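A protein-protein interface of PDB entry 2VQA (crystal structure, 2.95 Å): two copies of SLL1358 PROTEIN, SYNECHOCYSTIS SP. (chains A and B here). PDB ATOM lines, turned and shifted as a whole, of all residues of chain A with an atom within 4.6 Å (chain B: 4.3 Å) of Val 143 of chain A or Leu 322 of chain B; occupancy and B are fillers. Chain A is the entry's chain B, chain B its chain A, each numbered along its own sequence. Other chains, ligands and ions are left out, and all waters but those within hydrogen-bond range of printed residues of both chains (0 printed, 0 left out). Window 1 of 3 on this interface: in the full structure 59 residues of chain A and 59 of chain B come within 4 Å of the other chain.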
ATOM      1  N   GLU A  66      -1.916   3.931  -6.544  1.00  0.00           N
ATOM      2  CA  GLU A  66      -1.943   2.619  -7.189  1.00  0.00           C
ATOM      3  C   GLU A  66      -0.781   1.707  -6.818  1.00  0.00           C
ATOM      4  O   GLU A  66       0.271   2.165  -6.368  1.00  0.00           O
ATOM      5  CB  GLU A  66      -1.981   2.772  -8.699  1.00  0.00           C
ATOM      6  CG  GLU A  66      -0.768   3.471  -9.259  1.00  0.00           C
ATOM      7  CD  GLU A  66      -0.600   3.198 -10.738  1.00  0.00           C
ATOM      8  OE1 GLU A  66       0.043   4.018 -11.445  1.00  0.00           O
ATOM      9  OE2 GLU A  66      -1.122   2.150 -11.181  1.00  0.00           O
ATOM     10  N   LEU A  67      -0.992   0.407  -7.016  1.00  0.00           N
ATOM     11  CA  LEU A  67       0.044  -0.587  -6.837  1.00  0.00           C
ATOM     12  C   LEU A  67       1.332  -0.213  -7.589  1.00  0.00           C
ATOM     13  O   LEU A  67       1.354  -0.187  -8.813  1.00  0.00           O
ATOM     14  CB  LEU A  67      -0.471  -1.933  -7.330  1.00  0.00           C
ATOM     15  CG  LEU A  67      -1.542  -2.627  -6.491  1.00  0.00           C
ATOM     16  CD1 LEU A  67      -2.266  -3.656  -7.321  1.00  0.00           C
ATOM     17  CD2 LEU A  67      -0.957  -3.265  -5.239  1.00  0.00           C
ATOM     18  N   PHE A 141       7.598   2.819 -10.153  1.00  0.00           N
ATOM     19  CA  PHE A 141       7.234   1.821 -11.144  1.00  0.00           C
ATOM     20  C   PHE A 141       5.763   1.464 -10.978  1.00  0.00           C
ATOM     21  O   PHE A 141       5.378   0.782 -10.020  1.00  0.00           O
ATOM     22  CB  PHE A 141       8.134   0.585 -11.023  1.00  0.00           C
ATOM     23  CG  PHE A 141       9.519   0.784 -11.595  1.00  0.00           C
ATOM     24  CD1 PHE A 141       9.880   0.199 -12.804  1.00  0.00           C
ATOM     25  CD2 PHE A 141      10.459   1.573 -10.936  1.00  0.00           C
ATOM     26  CE1 PHE A 141      11.148   0.383 -13.335  1.00  0.00           C
ATOM     27  CE2 PHE A 141      11.717   1.767 -11.465  1.00  0.00           C
ATOM     28  CZ  PHE A 141      12.065   1.167 -12.665  1.00  0.00           C
ATOM     29  N   SER A 142       4.936   1.954 -11.895  1.00  0.00           N
ATOM     30  CA  SER A 142       3.486   1.774 -11.786  1.00  0.00           C
ATOM     31  C   SER A 142       3.016   0.499 -12.483  1.00  0.00           C
ATOM     32  O   SER A 142       3.369   0.265 -13.632  1.00  0.00           O
ATOM     33  CB  SER A 142       2.778   2.996 -12.371  1.00  0.00           C
ATOM     34  OG  SER A 142       1.622   2.596 -13.084  1.00  0.00           O
ATOM     35  N   VAL A 143       2.226  -0.328 -11.806  1.00  0.00           N
ATOM     36  CA  VAL A 143       1.739  -1.552 -12.432  1.00  0.00           C
ATOM     37  C   VAL A 143       0.899  -1.253 -13.670  1.00  0.00           C
ATOM     38  O   VAL A 143       0.902  -2.023 -14.627  1.00  0.00           O
ATOM     39  CB  VAL A 143       0.929  -2.428 -11.462  1.00  0.00           C
ATOM     40  CG1 VAL A 143      -0.488  -1.922 -11.322  1.00  0.00           C
ATOM     41  CG2 VAL A 143       0.905  -3.867 -11.935  1.00  0.00           C
ATOM     42  N   THR A 144       0.185  -0.132 -13.662  1.00  0.00           N
ATOM     43  CA  THR A 144      -0.631   0.214 -14.821  1.00  0.00           C
ATOM     44  C   THR A 144       0.249   0.683 -15.961  1.00  0.00           C
ATOM     45  O   THR A 144       0.082   0.230 -17.093  1.00  0.00           O
ATOM     46  CB  THR A 144      -1.706   1.281 -14.534  1.00  0.00           C
ATOM     47  OG1 THR A 144      -1.101   2.422 -13.918  1.00  0.00           O
ATOM     48  CG2 THR A 144      -2.809   0.715 -13.650  1.00  0.00           C
ATOM     49  N   ASP A 145       1.172   1.595 -15.653  1.00  0.00           N
ATOM     50  CA  ASP A 145       2.224   1.986 -16.587  1.00  0.00           C
ATOM     51  C   ASP A 145       2.879   0.705 -17.147  1.00  0.00           C
ATOM     52  O   ASP A 145       3.064   0.554 -18.361  1.00  0.00           O
ATOM     53  CB  ASP A 145       3.248   2.886 -15.871  1.00  0.00           C
ATOM     54  CG  ASP A 145       4.177   3.643 -16.836  1.00  0.00           C
ATOM     55  OD1 ASP A 145       3.771   3.948 -17.975  1.00  0.00           O
ATOM     56  OD2 ASP A 145       5.326   3.953 -16.446  1.00  0.00           O
ATOM     57  N   TRP A 146       3.187  -0.228 -16.245  1.00  0.00           N
ATOM     58  CA  TRP A 146       3.842  -1.477 -16.610  1.00  0.00           C
ATOM     59  C   TRP A 146       3.072  -2.204 -17.679  1.00  0.00           C
ATOM     60  O   TRP A 146       3.603  -2.426 -18.760  1.00  0.00           O
ATOM     61  CB  TRP A 146       4.036  -2.397 -15.406  1.00  0.00           C
ATOM     62  CG  TRP A 146       4.968  -3.522 -15.693  1.00  0.00           C
ATOM     63  CD1 TRP A 146       5.713  -3.698 -16.823  1.00  0.00           C
ATOM     64  CD2 TRP A 146       5.299  -4.612 -14.823  1.00  0.00           C
ATOM     65  NE1 TRP A 146       6.473  -4.840 -16.721  1.00  0.00           N
ATOM     66  CE2 TRP A 146       6.238  -5.418 -15.502  1.00  0.00           C
ATOM     67  CE3 TRP A 146       4.889  -4.988 -13.538  1.00  0.00           C
ATOM     68  CZ2 TRP A 146       6.775  -6.573 -14.939  1.00  0.00           C
ATOM     69  CZ3 TRP A 146       5.423  -6.137 -12.984  1.00  0.00           C
ATOM     70  CH2 TRP A 146       6.360  -6.914 -13.682  1.00  0.00           C
ATOM     71  N   LEU A 147       1.824  -2.565 -17.383  1.00  0.00           N
ATOM     72  CA  LEU A 147       1.018  -3.373 -18.308  1.00  0.00           C
ATOM     73  C   LEU A 147       0.646  -2.676 -19.627  1.00  0.00           C
ATOM     74  O   LEU A 147       0.380  -3.351 -20.627  1.00  0.00           O
ATOM     75  CB  LEU A 147      -0.228  -3.929 -17.617  1.00  0.00           C
ATOM     76  CG  LEU A 147       0.035  -4.956 -16.516  1.00  0.00           C
ATOM     77  CD1 LEU A 147      -1.219  -5.730 -16.213  1.00  0.00           C
ATOM     78  CD2 LEU A 147       1.169  -5.925 -16.886  1.00  0.00           C
ATOM     79  N   LEU A 159      -1.762 -13.263 -18.549  1.00  0.00           N
ATOM     80  CA  LEU A 159      -2.954 -13.211 -17.739  1.00  0.00           C
ATOM     81  C   LEU A 159      -3.959 -14.258 -18.150  1.00  0.00           C
ATOM     82  O   LEU A 159      -4.968 -14.412 -17.494  1.00  0.00           O
ATOM     83  CB  LEU A 159      -3.593 -11.834 -17.852  1.00  0.00           C
ATOM     84  CG  LEU A 159      -2.751 -10.698 -17.300  1.00  0.00           C
ATOM     85  CD1 LEU A 159      -3.525  -9.419 -17.506  1.00  0.00           C
ATOM     86  CD2 LEU A 159      -2.493 -10.930 -15.836  1.00  0.00           C
ATOM     87  N   LEU B 249       5.884 -11.850 -16.335  1.00  0.00           N
ATOM     88  CA  LEU B 249       6.365 -10.519 -15.957  1.00  0.00           C
ATOM     89  C   LEU B 249       6.811 -10.484 -14.495  1.00  0.00           C
ATOM     90  O   LEU B 249       6.100 -10.952 -13.610  1.00  0.00           O
ATOM     91  CB  LEU B 249       5.275  -9.472 -16.190  1.00  0.00           C
ATOM     92  CG  LEU B 249       4.940  -9.112 -17.630  1.00  0.00           C
ATOM     93  CD1 LEU B 249       3.496  -8.670 -17.733  1.00  0.00           C
ATOM     94  CD2 LEU B 249       5.880  -8.044 -18.141  1.00  0.00           C
ATOM     95  N   ILE B 320       9.679 -10.944  -7.723  1.00  0.00           N
ATOM     96  CA  ILE B 320       8.260 -10.704  -7.487  1.00  0.00           C
ATOM     97  C   ILE B 320       7.558 -10.776  -8.837  1.00  0.00           C
ATOM     98  O   ILE B 320       7.746  -9.879  -9.661  1.00  0.00           O
ATOM     99  CB  ILE B 320       8.015  -9.316  -6.862  1.00  0.00           C
ATOM    100  CG1 ILE B 320       8.803  -9.174  -5.548  1.00  0.00           C
ATOM    101  CG2 ILE B 320       6.510  -9.062  -6.675  1.00  0.00           C
ATOM    102  CD1 ILE B 320       8.330  -8.052  -4.643  1.00  0.00           C
ATOM    103  N   ASP B 321       6.788 -11.838  -9.084  1.00  0.00           N
ATOM    104  CA  ASP B 321       6.079 -11.984 -10.361  1.00  0.00           C
ATOM    105  C   ASP B 321       4.813 -11.159 -10.360  1.00  0.00           C
ATOM    106  O   ASP B 321       4.164 -11.009  -9.327  1.00  0.00           O
ATOM    107  CB  ASP B 321       5.688 -13.440 -10.650  1.00  0.00           C
ATOM    108  CG  ASP B 321       6.882 -14.342 -10.897  1.00  0.00           C
ATOM    109  OD1 ASP B 321       6.767 -15.564 -10.644  1.00  0.00           O
ATOM    110  OD2 ASP B 321       7.946 -13.845 -11.331  1.00  0.00           O
ATOM    111  N   LEU B 322       4.428 -10.657 -11.526  1.00  0.00           N
ATOM    112  CA  LEU B 322       3.241  -9.839 -11.595  1.00  0.00           C
ATOM    113  C   LEU B 322       2.089 -10.609 -10.989  1.00  0.00           C
ATOM    114  O   LEU B 322       1.359 -10.082 -10.153  1.00  0.00           O
ATOM    115  CB  LEU B 322       2.912  -9.456 -13.028  1.00  0.00           C
ATOM    116  CG  LEU B 322       1.568  -8.737 -13.115  1.00  0.00           C
ATOM    117  CD1 LEU B 322       1.682  -7.309 -12.592  1.00  0.00           C
ATOM    118  CD2 LEU B 322       1.077  -8.756 -14.530  1.00  0.00           C
ATOM    119  N   SER B 323       1.933 -11.863 -11.400  1.00  0.00           N
ATOM    120  CA  SER B 323       0.824 -12.673 -10.920  1.00  0.00           C
ATOM    121  C   SER B 323       0.794 -12.804  -9.399  1.00  0.00           C
ATOM    122  O   SER B 323      -0.257 -12.626  -8.780  1.00  0.00           O
ATOM    123  CB  SER B 323       0.877 -14.051 -11.549  1.00  0.00           C
ATOM    124  OG  SER B 323       2.211 -14.502 -11.543  1.00  0.00           O
ATOM    125  N   THR B 324       1.937 -13.122  -8.794  1.00  0.00           N
ATOM    126  CA  THR B 324       2.007 -13.242  -7.335  1.00  0.00           C
ATOM    127  C   THR B 324       1.551 -11.949  -6.676  1.00  0.00           C
ATOM    128  O   THR B 324       0.811 -11.958  -5.680  1.00  0.00           O
ATOM    129  CB  THR B 324       3.428 -13.518  -6.862  1.00  0.00           C
ATOM    130  OG1 THR B 324       3.782 -14.858  -7.199  1.00  0.00           O
ATOM    131  CG2 THR B 324       3.531 -13.339  -5.363  1.00  0.00           C
ATOM    132  N   TRP B 325       2.007 -10.837  -7.244  1.00  0.00           N
ATOM    133  CA  TRP B 325       1.698  -9.528  -6.716  1.00  0.00           C
ATOM    134  C   TRP B 325       0.202  -9.238  -6.761  1.00  0.00           C
ATOM    135  O   TRP B 325      -0.413  -8.943  -5.734  1.00  0.00           O
ATOM    136  CB  TRP B 325       2.489  -8.465  -7.456  1.00  0.00           C
ATOM    137  CG  TRP B 325       2.399  -7.124  -6.835  1.00  0.00           C
ATOM    138  CD1 TRP B 325       2.086  -6.833  -5.535  1.00  0.00           C
ATOM    139  CD2 TRP B 325       2.670  -5.875  -7.472  1.00  0.00           C
ATOM    140  NE1 TRP B 325       2.124  -5.476  -5.335  1.00  0.00           N
ATOM    141  CE2 TRP B 325       2.475  -4.865  -6.509  1.00  0.00           C
ATOM    142  CE3 TRP B 325       3.048  -5.511  -8.767  1.00  0.00           C
ATOM    143  CZ2 TRP B 325       2.641  -3.524  -6.799  1.00  0.00           C
ATOM    144  CZ3 TRP B 325       3.203  -4.187  -9.054  1.00  0.00           C
ATOM    145  CH2 TRP B 325       3.004  -3.202  -8.075  1.00  0.00           C
ATOM    146  N   LEU B 326      -0.384  -9.333  -7.949  1.00  0.00           N
ATOM    147  CA  LEU B 326      -1.817  -9.134  -8.104  1.00  0.00           C
ATOM    148  C   LEU B 326      -2.623 -10.103  -7.231  1.00  0.00           C
ATOM    149  O   LEU B 326      -3.540  -9.683  -6.538  1.00  0.00           O
ATOM    150  CB  LEU B 326      -2.209  -9.238  -9.572  1.00  0.00           C
ATOM    151  CG  LEU B 326      -1.553  -8.185 -10.471  1.00  0.00           C
ATOM    152  CD1 LEU B 326      -2.222  -8.149 -11.845  1.00  0.00           C
ATOM    153  CD2 LEU B 326      -1.546  -6.790  -9.823  1.00  0.00           C
ATOM    154  N   THR B 337      -7.140   0.206  -9.090  1.00  0.00           N
ATOM    155  CA  THR B 337      -5.870   0.482  -9.724  1.00  0.00           C
ATOM    156  C   THR B 337      -6.046   0.394 -11.234  1.00  0.00           C
ATOM    157  O   THR B 337      -5.691   1.314 -11.980  1.00  0.00           O
ATOM    158  CB  THR B 337      -4.821  -0.536  -9.270  1.00  0.00           C
ATOM    159  OG1 THR B 337      -4.595  -0.395  -7.856  1.00  0.00           O
ATOM    160  CG2 THR B 337      -3.527  -0.345 -10.036  1.00  0.00           C
ATOM    161  N   PHE B 338      -6.630  -0.712 -11.676  1.00  0.00           N
ATOM    162  CA  PHE B 338      -6.791  -0.949 -13.090  1.00  0.00           C
ATOM    163  C   PHE B 338      -8.030  -0.256 -13.693  1.00  0.00           C
ATOM    164  O   PHE B 338      -8.187  -0.218 -14.925  1.00  0.00           O
ATOM    165  CB  PHE B 338      -6.790  -2.453 -13.354  1.00  0.00           C
ATOM    166  CG  PHE B 338      -5.463  -3.117 -13.071  1.00  0.00           C
ATOM    167  CD1 PHE B 338      -4.346  -2.831 -13.851  1.00  0.00           C
ATOM    168  CD2 PHE B 338      -5.337  -4.038 -12.048  1.00  0.00           C
ATOM    169  CE1 PHE B 338      -3.133  -3.443 -13.601  1.00  0.00           C
ATOM    170  CE2 PHE B 338      -4.125  -4.661 -11.796  1.00  0.00           C
ATOM    171  CZ  PHE B 338      -3.026  -4.363 -12.569  1.00  0.00           C
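No position is printed for both chains.
The backbone carbonyl oxygen (O) of Leu 249 of chain B sits at hydrogen-bond distance from the backbone NH (N) of Leu 322 of chain B (2.7 Å).
The side-chain hydroxyl of Ser 142 of chain A sits at hydrogen-bond distance from the side-chain carboxylate of Glu 66 of chain A (2.7 Å).
The side-chain hydroxyl (OG1) of Thr 144 of chain A is in hydrogen-bond range of the side-chain carboxylate (OE2) of Glu 66 of chain A (2.8 Å).
The backbone NH (N) of Val 143 of chain A lies within hydrogen-bond range of the backbone carbonyl oxygen (O) of Leu 67 of chain A, 3.1 Å away.
The side-chain hydroxyl (OG) of Ser 142 of chain A sits at hydrogen-bond distance from the side-chain hydroxyl (OG1) of Thr 144 of chain A (2.9 Å).
Leu 67 of chain A touches Trp 325 of chain B (C to CH2, 3.5 Å).
CG2 of Val 143 of chain A touches CZ3 of Trp 325 of chain B, at 3.7 Å.
Val 143 of chain A touches Thr 337 of chain B.
Phe 338 of chain B touches Val 143 of chain A.
Thr 337 of chain B touches Thr 144 of chain A.
Thr 144 of chain A touches Phe 338 of chain B (CG2 to CD1, 3.9 Å).
Trp 146 of chain A touches Leu 249 of chain B.
Trp 146 of chain A touches Leu 322 of chain B (CZ3 to CD1, 3.9 Å).
Leu 249 of chain B touches Leu 147 of chain A (CD1 to CD2, 3.7 Å).
Leu 322 of chain B touches Leu 147 of chain A (CD2 to CD2, 3.7 Å).
Val 143 of chain A touches four residues of chain B.
Of the printed residues of chain A, Leu 322 of chain B touches Val 143 (3.6 Å), Trp 146 (3.9 Å) and Leu 147 (3.7 Å).
Of the printed residues of chain B, Thr 144 of chain A touches Thr 337 and Phe 338.
Printed residues of chain A within 4 Å of Leu 249 of chain B: Trp 146 and Leu 147.
Ser 323 of chain B touches none of the printed residues of chain A.
Phe 141 of chain A touches none of the printed residues of chain B.
The nearest printed residue of chain B that does not touch Val 143 of chain A is Leu 326 of chain B (4.4 Å).
The nearest printed residue of chain B that does not touch Leu 67 of chain A is Leu 326 of chain B (4.1 Å).
Of the 10 printed residues of chain B, 5 touch a printed residue of chain A.
Hydrophobic or aromatic side chains of chain B within 4 Å of the printed part of chain A: Leu 249, Leu 322, Trp 325 and Phe 338.
Printed residues of chain A that touch a printed residue of chain B: Glu 66, Leu 67, Val 143, Thr 144, Trp 146 and Leu 147.
Hydrophobic or aromatic side chains of chain A within 4 Å of the printed part of chain B: Leu 67, Val 143, Trp 146 and Leu 147.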
